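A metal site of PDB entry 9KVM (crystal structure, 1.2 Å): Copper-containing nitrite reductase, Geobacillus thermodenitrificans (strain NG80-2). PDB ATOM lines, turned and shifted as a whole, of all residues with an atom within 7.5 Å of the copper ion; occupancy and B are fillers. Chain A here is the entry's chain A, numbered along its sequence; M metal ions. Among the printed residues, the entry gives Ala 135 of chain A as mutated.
The backbone NH (N) of Met 148 sits close to the backbone carbonyl oxygen (O) of Trp 63 (3.2 Å).
The backbone carbonyl oxygen (O) of Asn 146 sits at hydrogen-bond distance from the backbone NH (N) of Trp 63.
The backbone carbonyl oxygen of Met 148 is in hydrogen-bond range of the backbone NH of Ala 135, at 3.3 Å.
OD2 of Asp 90 is in hydrogen-bond range of NE2 of His 95 (2.8 Å).
The backbone carbonyl oxygen (O) of Val 93 sits close to a ring nitrogen (NE2) of His 95 (3.3 Å).
Residues that only touch the copper ion: Trp 63 (3.99 Å) and Ala 135 (3.6 Å).
Five residues have an atom within 4 Å of the copper ion: Trp 63, His 95, Ala 135, His 143 and Met 148.
The nearest printed residue that does not touch the copper ion is Pro 94 (4.5 Å).
ND1 of His 143 binds the copper ion.
ND1 of His 95 is bound to the copper ion, at 2.1 Å.
SD of Met 148 binds the copper ion (2.2 Å).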
ATOM      1  N   ALA A  47       3.883 -29.519 -23.783  1.00  0.00           N
ATOM      2  CA  ALA A  47       2.469 -29.574 -23.450  1.00  0.00           C
ATOM      3  C   ALA A  47       2.343 -30.497 -22.252  1.00  0.00           C
ATOM      4  O   ALA A  47       2.865 -31.625 -22.292  1.00  0.00           O
ATOM      5  CB  ALA A  47       1.644 -30.107 -24.617  1.00  0.00           C
ATOM      6  N   ILE A  49       0.177 -31.309 -18.166  1.00  0.00           N
ATOM      7  CA  ILE A  49      -1.024 -31.206 -17.339  1.00  0.00           C
ATOM      8  C   ILE A  49      -0.573 -30.822 -15.945  1.00  0.00           C
ATOM      9  O   ILE A  49       0.171 -31.566 -15.308  1.00  0.00           O
ATOM     10  CB  ILE A  49      -1.754 -32.563 -17.341  1.00  0.00           C
ATOM     11  CG1 ILE A  49      -2.093 -33.017 -18.770  1.00  0.00           C
ATOM     12  CG2 ILE A  49      -2.974 -32.501 -16.446  1.00  0.00           C
ATOM     13  CD1 ILE A  49      -2.859 -32.000 -19.614  1.00  0.00           C
ATOM     14  N   TRP A  63      -4.595 -27.703 -18.905  1.00  0.00           N
ATOM     15  CA  TRP A  63      -3.841 -28.124 -20.064  1.00  0.00           C
ATOM     16  C   TRP A  63      -2.938 -26.962 -20.413  1.00  0.00           C
ATOM     17  O   TRP A  63      -3.424 -25.891 -20.754  1.00  0.00           O
ATOM     18  CB  TRP A  63      -4.781 -28.420 -21.232  1.00  0.00           C
ATOM     19  CG  TRP A  63      -5.764 -29.511 -21.014  1.00  0.00           C
ATOM     20  CD1 TRP A  63      -6.042 -30.168 -19.865  1.00  0.00           C
ATOM     21  CD2 TRP A  63      -6.625 -30.046 -22.023  1.00  0.00           C
ATOM     22  NE1 TRP A  63      -7.034 -31.101 -20.092  1.00  0.00           N
ATOM     23  CE2 TRP A  63      -7.408 -31.043 -21.413  1.00  0.00           C
ATOM     24  CE3 TRP A  63      -6.831 -29.749 -23.358  1.00  0.00           C
ATOM     25  CZ2 TRP A  63      -8.366 -31.784 -22.129  1.00  0.00           C
ATOM     26  CZ3 TRP A  63      -7.768 -30.458 -24.071  1.00  0.00           C
ATOM     27  CH2 TRP A  63      -8.527 -31.475 -23.455  1.00  0.00           C
ATOM     28  N   THR A  64      -1.629 -27.158 -20.297  1.00  0.00           N
ATOM     29  CA  THR A  64      -0.714 -26.021 -20.333  1.00  0.00           C
ATOM     30  C   THR A  64       0.422 -26.229 -21.316  1.00  0.00           C
ATOM     31  O   THR A  64       0.787 -27.355 -21.672  1.00  0.00           O
ATOM     32  CB  THR A  64      -0.063 -25.736 -18.962  1.00  0.00           C
ATOM     33  OG1 THR A  64       0.892 -26.755 -18.649  1.00  0.00           O
ATOM     34  CG2 THR A  64      -1.102 -25.638 -17.857  1.00  0.00           C
ATOM     35  N   PHE A  65       1.051 -25.101 -21.659  1.00  0.00           N
ATOM     36  CA  PHE A  65       2.419 -25.105 -22.147  1.00  0.00           C
ATOM     37  C   PHE A  65       3.348 -24.849 -20.963  1.00  0.00           C
ATOM     38  O   PHE A  65       3.216 -23.820 -20.278  1.00  0.00           O
ATOM     39  CB  PHE A  65       2.575 -24.015 -23.191  1.00  0.00           C
ATOM     40  CG  PHE A  65       1.731 -24.241 -24.415  1.00  0.00           C
ATOM     41  CD1 PHE A  65       2.035 -25.257 -25.304  1.00  0.00           C
ATOM     42  CD2 PHE A  65       0.658 -23.421 -24.681  1.00  0.00           C
ATOM     43  CE1 PHE A  65       1.270 -25.450 -26.449  1.00  0.00           C
ATOM     44  CE2 PHE A  65      -0.114 -23.594 -25.829  1.00  0.00           C
ATOM     45  CZ  PHE A  65       0.190 -24.623 -26.714  1.00  0.00           C
ATOM     46  N   ASN A  88       5.165 -33.237 -26.283  1.00  0.00           N
ATOM     47  CA  ASN A  88       3.865 -33.508 -25.655  1.00  0.00           C
ATOM     48  C   ASN A  88       4.023 -34.515 -24.525  1.00  0.00           C
ATOM     49  O   ASN A  88       4.288 -35.696 -24.769  1.00  0.00           O
ATOM     50  CB  ASN A  88       2.877 -34.020 -26.690  1.00  0.00           C
ATOM     51  CG  ASN A  88       1.479 -34.123 -26.132  1.00  0.00           C
ATOM     52  OD1 ASN A  88       1.262 -33.812 -24.963  1.00  0.00           O
ATOM     53  ND2 ASN A  88       0.531 -34.552 -26.945  1.00  0.00           N
ATOM     54  N   ASP A  90       1.533 -34.950 -22.271  1.00  0.00           N
ATOM     55  CA  ASP A  90       0.214 -35.441 -21.914  1.00  0.00           C
ATOM     56  C   ASP A  90       0.138 -36.925 -22.236  1.00  0.00           C
ATOM     57  O   ASP A  90       0.514 -37.317 -23.355  1.00  0.00           O
ATOM     58  CB  ASP A  90      -0.803 -34.659 -22.739  1.00  0.00           C
ATOM     59  CG  ASP A  90      -2.250 -34.918 -22.341  1.00  0.00           C
ATOM     60  OD1 ASP A  90      -2.653 -36.071 -22.080  1.00  0.00           O
ATOM     61  OD2 ASP A  90      -3.013 -33.935 -22.358  1.00  0.00           O
ATOM     62  N   VAL A  93      -3.896 -36.952 -24.679  1.00  0.00           N
ATOM     63  CA  VAL A  93      -4.472 -35.945 -25.568  1.00  0.00           C
ATOM     64  C   VAL A  93      -3.385 -35.373 -26.479  1.00  0.00           C
ATOM     65  O   VAL A  93      -2.355 -34.928 -25.976  1.00  0.00           O
ATOM     66  CB  VAL A  93      -5.193 -34.817 -24.784  1.00  0.00           C
ATOM     67  CG1 VAL A  93      -5.854 -33.848 -25.746  1.00  0.00           C
ATOM     68  CG2 VAL A  93      -6.219 -35.384 -23.811  1.00  0.00           C
ATOM     69  N   PRO A  94      -3.601 -35.320 -27.795  1.00  0.00           N
ATOM     70  CA  PRO A  94      -2.684 -34.570 -28.664  1.00  0.00           C
ATOM     71  C   PRO A  94      -2.779 -33.083 -28.409  1.00  0.00           C
ATOM     72  O   PRO A  94      -3.827 -32.563 -28.023  1.00  0.00           O
ATOM     73  CB  PRO A  94      -3.177 -34.909 -30.074  1.00  0.00           C
ATOM     74  CG  PRO A  94      -4.182 -35.968 -29.924  1.00  0.00           C
ATOM     75  CD  PRO A  94      -4.734 -35.874 -28.550  1.00  0.00           C
ATOM     76  N   HIS A  95      -1.670 -32.374 -28.680  1.00  0.00           N
ATOM     77  CA  HIS A  95      -1.654 -30.921 -28.598  1.00  0.00           C
ATOM     78  C   HIS A  95      -0.835 -30.379 -29.760  1.00  0.00           C
ATOM     79  O   HIS A  95      -0.132 -31.115 -30.444  1.00  0.00           O
ATOM     80  CB  HIS A  95      -1.121 -30.385 -27.253  1.00  0.00           C
ATOM     81  CG  HIS A  95      -1.864 -30.942 -26.078  1.00  0.00           C
ATOM     82  ND1 HIS A  95      -3.082 -30.460 -25.665  1.00  0.00           N
ATOM     83  CD2 HIS A  95      -1.551 -31.952 -25.231  1.00  0.00           C
ATOM     84  CE1 HIS A  95      -3.492 -31.154 -24.625  1.00  0.00           C
ATOM     85  NE2 HIS A  95      -2.568 -32.061 -24.329  1.00  0.00           N
ATOM     86  N   SER A  96      -0.927 -29.087 -29.980  1.00  0.00           N
ATOM     87  CA  SER A  96      -0.267 -28.424 -31.100  1.00  0.00           C
ATOM     88  C   SER A  96      -0.033 -26.968 -30.722  1.00  0.00           C
ATOM     89  O   SER A  96      -0.486 -26.512 -29.676  1.00  0.00           O
ATOM     90  CB  SER A  96      -1.136 -28.448 -32.360  1.00  0.00           C
ATOM     91  OG  SER A  96      -2.357 -27.786 -32.149  1.00  0.00           O
ATOM     92  N   HIS A 134      -1.672 -20.278 -29.094  1.00  0.00           N
ATOM     93  CA  HIS A 134      -2.586 -21.219 -28.470  1.00  0.00           C
ATOM     94  C   HIS A 134      -2.506 -22.549 -29.201  1.00  0.00           C
ATOM     95  O   HIS A 134      -1.981 -22.628 -30.302  1.00  0.00           O
ATOM     96  CB  HIS A 134      -4.046 -20.675 -28.464  1.00  0.00           C
ATOM     97  CG  HIS A 134      -4.600 -20.381 -29.823  1.00  0.00           C
ATOM     98  ND1 HIS A 134      -5.145 -21.341 -30.644  1.00  0.00           N
ATOM     99  CD2 HIS A 134      -4.703 -19.204 -30.499  1.00  0.00           C
ATOM    100  CE1 HIS A 134      -5.548 -20.779 -31.775  1.00  0.00           C
ATOM    101  NE2 HIS A 134      -5.292 -19.486 -31.705  1.00  0.00           N
ATOM    102  N   ALA A 135      -3.082 -23.572 -28.593  1.00  0.00           N
ATOM    103  CA  ALA A 135      -3.176 -24.855 -29.253  1.00  0.00           C
ATOM    104  C   ALA A 135      -4.170 -24.778 -30.412  1.00  0.00           C
ATOM    105  O   ALA A 135      -5.149 -24.044 -30.364  1.00  0.00           O
ATOM    106  CB  ALA A 135      -3.619 -25.951 -28.285  1.00  0.00           C
ATOM    107  N   GLY A 136      -3.877 -25.530 -31.465  1.00  0.00           N
ATOM    108  CA  GLY A 136      -4.688 -25.580 -32.665  1.00  0.00           C
ATOM    109  C   GLY A 136      -5.425 -26.888 -32.838  1.00  0.00           C
ATOM    110  O   GLY A 136      -5.974 -27.126 -33.916  1.00  0.00           O
ATOM    111  N   THR A 137      -5.478 -27.730 -31.815  1.00  0.00           N
ATOM    112  CA  THR A 137      -6.051 -29.065 -31.901  1.00  0.00           C
ATOM    113  C   THR A 137      -7.561 -28.980 -31.712  1.00  0.00           C
ATOM    114  O   THR A 137      -8.057 -28.277 -30.832  1.00  0.00           O
ATOM    115  CB  THR A 137      -5.434 -29.895 -30.772  1.00  0.00           C
ATOM    116  OG1 THR A 137      -4.013 -29.889 -30.933  1.00  0.00           O
ATOM    117  CG2 THR A 137      -5.913 -31.338 -30.757  1.00  0.00           C
ATOM    118  N   PRO A 139     -11.224 -29.963 -30.481  1.00  0.00           N
ATOM    119  CA  PRO A 139     -11.867 -28.640 -30.647  1.00  0.00           C
ATOM    120  C   PRO A 139     -11.002 -27.558 -30.031  1.00  0.00           C
ATOM    121  O   PRO A 139     -10.632 -27.653 -28.848  1.00  0.00           O
ATOM    122  CB  PRO A 139     -13.190 -28.777 -29.873  1.00  0.00           C
ATOM    123  CG  PRO A 139     -13.226 -30.168 -29.342  1.00  0.00           C
ATOM    124  CD  PRO A 139     -11.852 -30.728 -29.393  1.00  0.00           C
ATOM    125  N   VAL A 140     -10.674 -26.543 -30.815  1.00  0.00           N
ATOM    126  CA  VAL A 140      -9.773 -25.488 -30.335  1.00  0.00           C
ATOM    127  C   VAL A 140     -10.326 -24.830 -29.069  1.00  0.00           C
ATOM    128  O   VAL A 140      -9.582 -24.555 -28.133  1.00  0.00           O
ATOM    129  CB  VAL A 140      -9.484 -24.480 -31.466  1.00  0.00           C
ATOM    130  CG1 VAL A 140      -8.652 -23.303 -30.955  1.00  0.00           C
ATOM    131  CG2 VAL A 140      -8.783 -25.171 -32.612  1.00  0.00           C
ATOM    132  N   GLN A 142     -11.879 -26.101 -26.638  1.00  0.00           N
ATOM    133  CA  GLN A 142     -11.566 -26.904 -25.460  1.00  0.00           C
ATOM    134  C   GLN A 142     -10.129 -26.722 -24.999  1.00  0.00           C
ATOM    135  O   GLN A 142      -9.864 -26.600 -23.806  1.00  0.00           O
ATOM    136  CB  GLN A 142     -11.826 -28.380 -25.773  1.00  0.00           C
ATOM    137  CG  GLN A 142     -11.691 -29.268 -24.576  1.00  0.00           C
ATOM    138  CD  GLN A 142     -12.074 -30.696 -24.877  1.00  0.00           C
ATOM    139  OE1 GLN A 142     -12.123 -31.102 -26.048  1.00  0.00           O
ATOM    140  NE2 GLN A 142     -12.317 -31.483 -23.834  1.00  0.00           N
ATOM    141  N   HIS A 143      -9.186 -26.688 -25.947  1.00  0.00           N
ATOM    142  CA  HIS A 143      -7.788 -26.497 -25.586  1.00  0.00           C
ATOM    143  C   HIS A 143      -7.540 -25.098 -25.036  1.00  0.00           C
ATOM    144  O   HIS A 143      -6.823 -24.967 -24.033  1.00  0.00           O
ATOM    145  CB  HIS A 143      -6.882 -26.787 -26.777  1.00  0.00           C
ATOM    146  CG  HIS A 143      -6.843 -28.231 -27.109  1.00  0.00           C
ATOM    147  ND1 HIS A 143      -5.766 -29.026 -26.806  1.00  0.00           N
ATOM    148  CD2 HIS A 143      -7.763 -29.028 -27.689  1.00  0.00           C
ATOM    149  CE1 HIS A 143      -6.017 -30.261 -27.206  1.00  0.00           C
ATOM    150  NE2 HIS A 143      -7.227 -30.291 -27.743  1.00  0.00           N
ATOM    151  N   ILE A 144      -8.116 -24.066 -25.644  1.00  0.00           N
ATOM    152  CA  ILE A 144      -7.907 -22.712 -25.120  1.00  0.00           C
ATOM    153  C   ILE A 144      -8.523 -22.583 -23.736  1.00  0.00           C
ATOM    154  O   ILE A 144      -7.874 -22.107 -22.800  1.00  0.00           O
ATOM    155  CB  ILE A 144      -8.440 -21.629 -26.063  1.00  0.00           C
ATOM    156  CG1 ILE A 144      -7.703 -21.664 -27.420  1.00  0.00           C
ATOM    157  CG2 ILE A 144      -8.254 -20.262 -25.405  1.00  0.00           C
ATOM    158  CD1 ILE A 144      -8.309 -20.715 -28.461  1.00  0.00           C
ATOM    159  N   ASN A 146      -9.135 -24.711 -21.480  1.00  0.00           N
ATOM    160  CA  ASN A 146      -8.461 -25.486 -20.455  1.00  0.00           C
ATOM    161  C   ASN A 146      -7.066 -24.952 -20.123  1.00  0.00           C
ATOM    162  O   ASN A 146      -6.433 -25.473 -19.209  1.00  0.00           O
ATOM    163  CB  ASN A 146      -8.372 -26.960 -20.826  1.00  0.00           C
ATOM    164  CG  ASN A 146      -9.673 -27.720 -20.572  1.00  0.00           C
ATOM    165  OD1 ASN A 146     -10.439 -27.408 -19.652  1.00  0.00           O
ATOM    166  ND2 ASN A 146      -9.907 -28.724 -21.371  1.00  0.00           N
ATOM    167  N   GLY A 147      -6.594 -23.902 -20.804  1.00  0.00           N
ATOM    168  CA  GLY A 147      -5.375 -23.226 -20.404  1.00  0.00           C
ATOM    169  C   GLY A 147      -4.301 -23.065 -21.477  1.00  0.00           C
ATOM    170  O   GLY A 147      -3.257 -22.479 -21.184  1.00  0.00           O
ATOM    171  N   MET A 148      -4.529 -23.545 -22.699  1.00  0.00           N
ATOM    172  CA  MET A 148      -3.450 -23.556 -23.701  1.00  0.00           C
ATOM    173  C   MET A 148      -3.457 -22.281 -24.522  1.00  0.00           C
ATOM    174  O   MET A 148      -3.877 -22.250 -25.685  1.00  0.00           O
ATOM    175  CB  MET A 148      -3.529 -24.785 -24.603  1.00  0.00           C
ATOM    176  CG  MET A 148      -3.099 -26.017 -23.922  1.00  0.00           C
ATOM    177  SD  MET A 148      -2.550 -27.295 -25.096  1.00  0.00           S
ATOM    178  CE  MET A 148      -1.431 -28.149 -24.012  1.00  0.00           C
HETATM  179 CU    CU M   1      -4.018 -28.620 -25.954  1.00  0.00          CU
